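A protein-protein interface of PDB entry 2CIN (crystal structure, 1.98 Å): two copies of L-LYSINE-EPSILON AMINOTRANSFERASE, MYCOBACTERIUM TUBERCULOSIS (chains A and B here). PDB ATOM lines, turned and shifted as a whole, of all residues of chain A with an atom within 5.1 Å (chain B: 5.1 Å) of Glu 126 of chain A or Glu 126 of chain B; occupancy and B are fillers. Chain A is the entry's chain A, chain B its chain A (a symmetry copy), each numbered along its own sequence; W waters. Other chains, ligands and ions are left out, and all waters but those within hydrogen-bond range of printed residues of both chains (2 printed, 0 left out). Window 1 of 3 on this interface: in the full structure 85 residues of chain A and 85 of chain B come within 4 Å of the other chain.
Printed residues of chain B within 4 Å of Lys 92 of chain A: Asp 337 (2.8 Å).
Glu 126 of chain A touches just these residues of chain B: Glu 126 and Gly 127.
Of the printed residues of chain B, Cys 305 of chain A touches Trp 331.
Printed residues of chain B within 4 Å of Trp 331 of chain A: Cys 305 (3.8 Å).
Glu 126 of chain B touches just these residues of chain A: Glu 126 (3.7 Å) and Gly 127 (3.6 Å).
Of the printed residues of chain A, Gly 127 of chain B touches Glu 126.
Of the printed residues of chain A, Asn 334 of chain B touches Asn 334 and Asp 337.
The nearest residue of chain B that does not touch Glu 126 of chain A is Asp 337 of chain B (4.04 Å).
The nearest printed residue of chain A that does not touch Asp 337 of chain B is Glu 126 of chain A (4.04 Å).
Water W1 lies within hydrogen-bond range of OE1 of Glu 126 of chain B (2.9 Å), N of Gly 127 of chain A (3.2 Å), NZ of Lys 92 of chain B (3.4 Å) and SG of Cys 305 of chain A (3.8 Å).
Water W2 lies within hydrogen-bond range of the side-chain carboxylate (OE1) of Glu 126 of chain A (2.9 Å), the backbone NH (N) of Gly 127 of chain B (3.2 Å), the side-chain amino group (NZ) of Lys 92 of chain A (3.4 Å) and the side-chain sulfur (SG) of Cys 305 of chain B (3.8 Å).
Lys 92 of chain A touches Asp 337 of chain B, and with the chains exchanged Asp 337 of chain A touches Lys 92 of chain B.
Glu 126 of chain A touches its own counterpart, Glu 126 of chain B.
Leu 130 of chain A touches its own counterpart, Leu 130 of chain B.
Asn 334 of chain A touches its own counterpart, Asn 334 of chain B.
Glu 126 of chain A touches Glu 126 of chain B.
OE1 of Glu 126 of chain A touches N of Gly 127 of chain B (3.6 Å).
Gly 127 of chain A touches Glu 126 of chain B.
CD1 of Leu 130 of chain B touches CD1 of Leu 130 of chain A, at 3.7 Å.
Cys 305 of chain A touches Trp 331 of chain B.
CZ3 of Trp 331 of chain A touches SG of Cys 305 of chain B (3.8 Å).
The side-chain amide nitrogen of Asn 334 of chain A is in hydrogen-bond range of the side-chain carboxylate of Asp 337 of chain B (3.0 Å).
ND2 of Asn 334 of chain B sits close to ND2 of Asn 334 of chain A, 3.2 Å away.
NZ of Lys 92 of chain A lies within salt-bridge range of OD2 of Asp 337 of chain B, at 2.8 Å.
OD2 of Asp 337 of chain A lies within hydrogen-bond range of ND2 of Asn 334 of chain B, 3.0 Å away.
OD2 of Asp 337 of chain A is in salt-bridge range of NZ of Lys 92 of chain B (2.8 Å).
N of Val 125 of chain B lies within hydrogen-bond range of O of Cys 305 of chain B (2.9 Å).
The side-chain amide nitrogen (ND2) of Asn 334 of chain B is in hydrogen-bond range of the side-chain carboxylate (OE2) of Glu 126 of chain B (3.4 Å).
The backbone NH (N) of Gly 128 of chain B lies within hydrogen-bond range of the side-chain sulfur (SG) of Cys 305 of chain B (3.6 Å).
The backbone NH (N) of Val 125 of chain A lies within hydrogen-bond range of the backbone carbonyl oxygen (O) of Cys 305 of chain A, 2.9 Å away.
The backbone NH of Gly 127 of chain A lies close to the side-chain sulfur of Cys 305 of chain A, at 3.5 Å.
The side-chain amino group (NZ) of Lys 92 of chain A is in salt-bridge range of the side-chain carboxylate (OE2) of Glu 126 of chain A, at 2.7 Å.
Of the 12 printed residues of chain A, 8 touch a printed residue of chain B.
Printed residues of chain A that touch a printed residue of chain B: Lys 92, Glu 126, Gly 127, Leu 130, Cys 305, Trp 331, Asn 334 and Asp 337.
Of the 12 printed residues of chain B, 8 touch a printed residue of chain A.
Hydrophobic or aromatic side chains of chain B that line the printed part of chain A: Leu 130 and Trp 331.
Among the printed residues, 11 pairs touch across the chains.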
ATOM      1  N   LYS A  92       5.991   3.283 -15.090  1.00  0.00           N
ATOM      2  CA  LYS A  92       7.022   2.349 -15.562  1.00  0.00           C
ATOM      3  C   LYS A  92       8.360   3.088 -15.623  1.00  0.00           C
ATOM      4  O   LYS A  92       8.742   3.634 -16.663  1.00  0.00           O
ATOM      5  CB  LYS A  92       6.632   1.729 -16.917  1.00  0.00           C
ATOM      6  CG  LYS A  92       7.576   0.628 -17.384  1.00  0.00           C
ATOM      7  CD  LYS A  92       7.167   0.023 -18.737  1.00  0.00           C
ATOM      8  CE  LYS A  92       8.019  -1.229 -18.982  1.00  0.00           C
ATOM      9  NZ  LYS A  92       7.697  -1.882 -20.280  1.00  0.00           N
ATOM     10  N   PHE A 124      19.391  -7.184 -15.577  1.00  0.00           N
ATOM     11  CA  PHE A 124      17.972  -7.444 -15.897  1.00  0.00           C
ATOM     12  C   PHE A 124      17.538  -6.730 -17.160  1.00  0.00           C
ATOM     13  O   PHE A 124      18.048  -5.646 -17.508  1.00  0.00           O
ATOM     14  CB  PHE A 124      17.080  -7.038 -14.726  1.00  0.00           C
ATOM     15  CG  PHE A 124      17.431  -7.769 -13.474  1.00  0.00           C
ATOM     16  CD1 PHE A 124      17.050  -9.102 -13.321  1.00  0.00           C
ATOM     17  CD2 PHE A 124      18.227  -7.165 -12.494  1.00  0.00           C
ATOM     18  CE1 PHE A 124      17.420  -9.839 -12.181  1.00  0.00           C
ATOM     19  CE2 PHE A 124      18.588  -7.899 -11.326  1.00  0.00           C
ATOM     20  CZ  PHE A 124      18.180  -9.227 -11.194  1.00  0.00           C
ATOM     21  N   VAL A 125      16.561  -7.332 -17.818  1.00  0.00           N
ATOM     22  CA  VAL A 125      16.084  -6.869 -19.125  1.00  0.00           C
ATOM     23  C   VAL A 125      14.680  -7.516 -19.347  1.00  0.00           C
ATOM     24  O   VAL A 125      14.343  -8.538 -18.720  1.00  0.00           O
ATOM     25  CB  VAL A 125      17.093  -7.265 -20.250  1.00  0.00           C
ATOM     26  CG1 VAL A 125      17.105  -8.778 -20.458  1.00  0.00           C
ATOM     27  CG2 VAL A 125      16.804  -6.540 -21.549  1.00  0.00           C
ATOM     28  N   GLU A 126      13.857  -6.894 -20.185  1.00  0.00           N
ATOM     29  CA  GLU A 126      12.606  -7.535 -20.608  1.00  0.00           C
ATOM     30  C   GLU A 126      12.910  -8.536 -21.725  1.00  0.00           C
ATOM     31  O   GLU A 126      13.502  -8.161 -22.747  1.00  0.00           O
ATOM     32  CB  GLU A 126      11.632  -6.480 -21.146  1.00  0.00           C
ATOM     33  CG  GLU A 126      11.094  -5.506 -20.107  1.00  0.00           C
ATOM     34  CD  GLU A 126      10.049  -4.527 -20.713  1.00  0.00           C
ATOM     35  OE1 GLU A 126      10.177  -4.149 -21.904  1.00  0.00           O
ATOM     36  OE2 GLU A 126       9.116  -4.143 -19.992  1.00  0.00           O
ATOM     37  N   GLY A 127      12.515  -9.795 -21.530  1.00  0.00           N
ATOM     38  CA  GLY A 127      12.467 -10.756 -22.624  1.00  0.00           C
ATOM     39  C   GLY A 127      13.590 -11.793 -22.525  1.00  0.00           C
ATOM     40  O   GLY A 127      14.737 -11.450 -22.242  1.00  0.00           O
ATOM     41  N   GLY A 128      13.235 -13.062 -22.739  1.00  0.00           N
ATOM     42  CA  GLY A 128      14.195 -14.161 -22.621  1.00  0.00           C
ATOM     43  C   GLY A 128      15.259 -14.182 -23.723  1.00  0.00           C
ATOM     44  O   GLY A 128      16.432 -14.490 -23.467  1.00  0.00           O
ATOM     45  N   LEU A 130      16.549 -11.620 -25.228  1.00  0.00           N
ATOM     46  CA  LEU A 130      17.499 -10.564 -24.881  1.00  0.00           C
ATOM     47  C   LEU A 130      18.382 -10.901 -23.653  1.00  0.00           C
ATOM     48  O   LEU A 130      19.523 -10.457 -23.580  1.00  0.00           O
ATOM     49  CB  LEU A 130      16.765  -9.239 -24.709  1.00  0.00           C
ATOM     50  CG  LEU A 130      17.041  -8.208 -25.823  1.00  0.00           C
ATOM     51  CD1 LEU A 130      17.186  -8.811 -27.215  1.00  0.00           C
ATOM     52  CD2 LEU A 130      16.034  -7.095 -25.827  1.00  0.00           C
ATOM     53  N   CYS A 305      13.577 -10.760 -16.960  1.00  0.00           N
ATOM     54  CA  CYS A 305      14.597 -11.665 -17.470  1.00  0.00           C
ATOM     55  C   CYS A 305      15.993 -11.103 -17.205  1.00  0.00           C
ATOM     56  O   CYS A 305      16.134  -9.987 -16.701  1.00  0.00           O
ATOM     57  CB  CYS A 305      14.358 -11.908 -18.965  1.00  0.00           C
ATOM     58  SG  CYS A 305      12.671 -12.499 -19.248  1.00  0.00           S
ATOM     59  N   TRP A 331      14.328   0.411 -20.157  1.00  0.00           N
ATOM     60  CA  TRP A 331      13.679   0.180 -18.868  1.00  0.00           C
ATOM     61  C   TRP A 331      14.482  -0.587 -17.819  1.00  0.00           C
ATOM     62  O   TRP A 331      14.238  -0.408 -16.607  1.00  0.00           O
ATOM     63  CB  TRP A 331      12.302  -0.461 -19.052  1.00  0.00           C
ATOM     64  CG  TRP A 331      11.283   0.544 -19.596  1.00  0.00           C
ATOM     65  CD1 TRP A 331      10.895   1.727 -19.024  1.00  0.00           C
ATOM     66  CD2 TRP A 331      10.517   0.409 -20.811  1.00  0.00           C
ATOM     67  NE1 TRP A 331       9.926   2.343 -19.810  1.00  0.00           N
ATOM     68  CE2 TRP A 331       9.671   1.550 -20.905  1.00  0.00           C
ATOM     69  CE3 TRP A 331      10.440  -0.581 -21.802  1.00  0.00           C
ATOM     70  CZ2 TRP A 331       8.774   1.742 -21.980  1.00  0.00           C
ATOM     71  CZ3 TRP A 331       9.542  -0.386 -22.882  1.00  0.00           C
ATOM     72  CH2 TRP A 331       8.725   0.762 -22.949  1.00  0.00           C
ATOM     73  N   GLY A 333      14.274  -3.835 -17.428  1.00  0.00           N
ATOM     74  CA  GLY A 333      13.292  -4.776 -16.867  1.00  0.00           C
ATOM     75  C   GLY A 333      12.045  -4.013 -16.419  1.00  0.00           C
ATOM     76  O   GLY A 333      12.091  -2.806 -16.211  1.00  0.00           O
ATOM     77  N   ASN A 334      10.927  -4.702 -16.308  1.00  0.00           N
ATOM     78  CA  ASN A 334       9.670  -4.081 -15.926  1.00  0.00           C
ATOM     79  C   ASN A 334       9.543  -4.046 -14.385  1.00  0.00           C
ATOM     80  O   ASN A 334       9.579  -5.089 -13.743  1.00  0.00           O
ATOM     81  CB  ASN A 334       8.518  -4.866 -16.573  1.00  0.00           C
ATOM     82  CG  ASN A 334       7.203  -4.122 -16.543  1.00  0.00           C
ATOM     83  OD1 ASN A 334       6.761  -3.653 -15.493  1.00  0.00           O
ATOM     84  ND2 ASN A 334       6.557  -4.017 -17.699  1.00  0.00           N
ATOM     85  N   ASP A 337       6.936  -6.404 -12.902  1.00  0.00           N
ATOM     86  CA  ASP A 337       7.469  -7.773 -12.901  1.00  0.00           C
ATOM     87  C   ASP A 337       8.420  -8.039 -11.740  1.00  0.00           C
ATOM     88  O   ASP A 337       8.392  -9.134 -11.154  1.00  0.00           O
ATOM     89  CB  ASP A 337       8.193  -8.080 -14.230  1.00  0.00           C
ATOM     90  CG  ASP A 337       7.219  -8.257 -15.389  1.00  0.00           C
ATOM     91  OD1 ASP A 337       6.002  -8.447 -15.166  1.00  0.00           O
ATOM     92  OD2 ASP A 337       7.676  -8.207 -16.524  1.00  0.00           O
ATOM     93  N   LYS B  92       0.917 -12.778 -15.264  1.00  0.00           N
ATOM     94  CA  LYS B  92       1.510 -12.338 -16.533  1.00  0.00           C
ATOM     95  C   LYS B  92       1.223 -13.398 -17.600  1.00  0.00           C
ATOM     96  O   LYS B  92       2.028 -14.304 -17.833  1.00  0.00           O
ATOM     97  CB  LYS B  92       3.017 -12.058 -16.377  1.00  0.00           C
ATOM     98  CG  LYS B  92       3.659 -11.440 -17.611  1.00  0.00           C
ATOM     99  CD  LYS B  92       5.162 -11.167 -17.431  1.00  0.00           C
ATOM    100  CE  LYS B  92       5.643 -10.322 -18.617  1.00  0.00           C
ATOM    101  NZ  LYS B  92       7.097 -10.013 -18.533  1.00  0.00           N
ATOM    102  N   PHE B 124       2.768  -6.953 -31.138  1.00  0.00           N
ATOM    103  CA  PHE B 124       3.299  -6.422 -29.864  1.00  0.00           C
ATOM    104  C   PHE B 124       4.360  -7.327 -29.274  1.00  0.00           C
ATOM    105  O   PHE B 124       4.343  -8.561 -29.456  1.00  0.00           O
ATOM    106  CB  PHE B 124       2.166  -6.211 -28.863  1.00  0.00           C
ATOM    107  CG  PHE B 124       1.129  -5.272 -29.378  1.00  0.00           C
ATOM    108  CD1 PHE B 124       1.385  -3.901 -29.398  1.00  0.00           C
ATOM    109  CD2 PHE B 124      -0.059  -5.757 -29.938  1.00  0.00           C
ATOM    110  CE1 PHE B 124       0.455  -2.993 -29.937  1.00  0.00           C
ATOM    111  CE2 PHE B 124      -1.015  -4.841 -30.467  1.00  0.00           C
ATOM    112  CZ  PHE B 124      -0.737  -3.474 -30.459  1.00  0.00           C
ATOM    113  N   VAL B 125       5.259  -6.701 -28.532  1.00  0.00           N
ATOM    114  CA  VAL B 125       6.436  -7.377 -27.975  1.00  0.00           C
ATOM    115  C   VAL B 125       6.975  -6.467 -26.827  1.00  0.00           C
ATOM    116  O   VAL B 125       6.690  -5.255 -26.785  1.00  0.00           O
ATOM    117  CB  VAL B 125       7.509  -7.615 -29.085  1.00  0.00           C
ATOM    118  CG1 VAL B 125       8.116  -6.291 -29.542  1.00  0.00           C
ATOM    119  CG2 VAL B 125       8.586  -8.579 -28.631  1.00  0.00           C
ATOM    120  N   GLU B 126       7.698  -7.058 -25.881  1.00  0.00           N
ATOM    121  CA  GLU B 126       8.411  -6.254 -24.882  1.00  0.00           C
ATOM    122  C   GLU B 126       9.717  -5.743 -25.493  1.00  0.00           C
ATOM    123  O   GLU B 126      10.530  -6.545 -25.976  1.00  0.00           O
ATOM    124  CB  GLU B 126       8.745  -7.114 -23.657  1.00  0.00           C
ATOM    125  CG  GLU B 126       7.546  -7.559 -22.832  1.00  0.00           C
ATOM    126  CD  GLU B 126       7.974  -8.350 -21.563  1.00  0.00           C
ATOM    127  OE1 GLU B 126       8.996  -9.079 -21.607  1.00  0.00           O
ATOM    128  OE2 GLU B 126       7.281  -8.240 -20.541  1.00  0.00           O
ATOM    129  N   GLY B 127       9.916  -4.424 -25.477  1.00  0.00           N
ATOM    130  CA  GLY B 127      11.229  -3.847 -25.738  1.00  0.00           C
ATOM    131  C   GLY B 127      11.293  -3.172 -27.111  1.00  0.00           C
ATOM    132  O   GLY B 127      10.805  -3.716 -28.101  1.00  0.00           O
ATOM    133  N   GLY B 128      11.881  -1.974 -27.147  1.00  0.00           N
ATOM    134  CA  GLY B 128      11.962  -1.192 -28.381  1.00  0.00           C
ATOM    135  C   GLY B 128      12.905  -1.782 -29.434  1.00  0.00           C
ATOM    136  O   GLY B 128      12.617  -1.742 -30.639  1.00  0.00           O
ATOM    137  N   LEU B 130      13.511  -4.919 -29.961  1.00  0.00           N
ATOM    138  CA  LEU B 130      12.788  -6.046 -30.553  1.00  0.00           C
ATOM    139  C   LEU B 130      11.610  -5.619 -31.465  1.00  0.00           C
ATOM    140  O   LEU B 130      11.296  -6.314 -32.424  1.00  0.00           O
ATOM    141  CB  LEU B 130      12.345  -7.012 -29.462  1.00  0.00           C
ATOM    142  CG  LEU B 130      13.100  -8.357 -29.454  1.00  0.00           C
ATOM    143  CD1 LEU B 130      14.580  -8.248 -29.805  1.00  0.00           C
ATOM    144  CD2 LEU B 130      12.911  -9.106 -28.166  1.00  0.00           C
ATOM    145  N   CYS B 305       5.692  -2.497 -26.654  1.00  0.00           N
ATOM    146  CA  CYS B 305       6.315  -2.091 -27.906  1.00  0.00           C
ATOM    147  C   CYS B 305       5.757  -2.908 -29.070  1.00  0.00           C
ATOM    148  O   CYS B 305       4.957  -3.824 -28.868  1.00  0.00           O
ATOM    149  CB  CYS B 305       7.836  -2.239 -27.786  1.00  0.00           C
ATOM    150  SG  CYS B 305       8.450  -1.322 -26.353  1.00  0.00           S
ATOM    151  N   TRP B 331       5.638 -13.880 -24.204  1.00  0.00           N
ATOM    152  CA  TRP B 331       4.538 -13.116 -23.617  1.00  0.00           C
ATOM    153  C   TRP B 331       3.656 -12.326 -24.582  1.00  0.00           C
ATOM    154  O   TRP B 331       2.474 -12.071 -24.264  1.00  0.00           O
ATOM    155  CB  TRP B 331       5.038 -12.208 -22.492  1.00  0.00           C
ATOM    156  CG  TRP B 331       5.396 -13.012 -21.238  1.00  0.00           C
ATOM    157  CD1 TRP B 331       4.570 -13.826 -20.509  1.00  0.00           C
ATOM    158  CD2 TRP B 331       6.677 -13.034 -20.577  1.00  0.00           C
ATOM    159  NE1 TRP B 331       5.259 -14.357 -19.423  1.00  0.00           N
ATOM    160  CE2 TRP B 331       6.550 -13.879 -19.438  1.00  0.00           C
ATOM    161  CE3 TRP B 331       7.903 -12.394 -20.816  1.00  0.00           C
ATOM    162  CZ2 TRP B 331       7.623 -14.125 -18.552  1.00  0.00           C
ATOM    163  CZ3 TRP B 331       8.979 -12.643 -19.930  1.00  0.00           C
ATOM    164  CH2 TRP B 331       8.820 -13.495 -18.816  1.00  0.00           C
ATOM    165  N   GLY B 333       4.184  -9.175 -25.317  1.00  0.00           N
ATOM    166  CA  GLY B 333       4.011  -7.882 -24.638  1.00  0.00           C
ATOM    167  C   GLY B 333       3.511  -8.114 -23.211  1.00  0.00           C
ATOM    168  O   GLY B 333       2.979  -9.173 -22.899  1.00  0.00           O
ATOM    169  N   ASN B 334       3.713  -7.146 -22.339  1.00  0.00           N
ATOM    170  CA  ASN B 334       3.315  -7.264 -20.947  1.00  0.00           C
ATOM    171  C   ASN B 334       1.846  -6.813 -20.775  1.00  0.00           C
ATOM    172  O   ASN B 334       1.511  -5.679 -21.096  1.00  0.00           O
ATOM    173  CB  ASN B 334       4.272  -6.419 -20.090  1.00  0.00           C
ATOM    174  CG  ASN B 334       4.184  -6.736 -18.615  1.00  0.00           C
ATOM    175  OD1 ASN B 334       3.101  -6.741 -18.029  1.00  0.00           O
ATOM    176  ND2 ASN B 334       5.332  -6.994 -17.997  1.00  0.00           N
ATOM    177  N   ASP B 337       1.350  -3.511 -18.930  1.00  0.00           N
ATOM    178  CA  ASP B 337       1.663  -2.399 -19.838  1.00  0.00           C
ATOM    179  C   ASP B 337       0.522  -2.075 -20.794  1.00  0.00           C
ATOM    180  O   ASP B 337       0.261  -0.892 -21.071  1.00  0.00           O
ATOM    181  CB  ASP B 337       2.938  -2.701 -20.654  1.00  0.00           C
ATOM    182  CG  ASP B 337       4.201  -2.611 -19.804  1.00  0.00           C
ATOM    183  OD1 ASP B 337       4.171  -2.042 -18.689  1.00  0.00           O
ATOM    184  OD2 ASP B 337       5.222  -3.112 -20.256  1.00  0.00           O
HETATM  185  O   HOH W   1      10.410  -9.488 -19.131  1.00  0.00           O
HETATM  186  O   HOH W   2       7.767  -3.437 -23.311  1.00  0.00           O
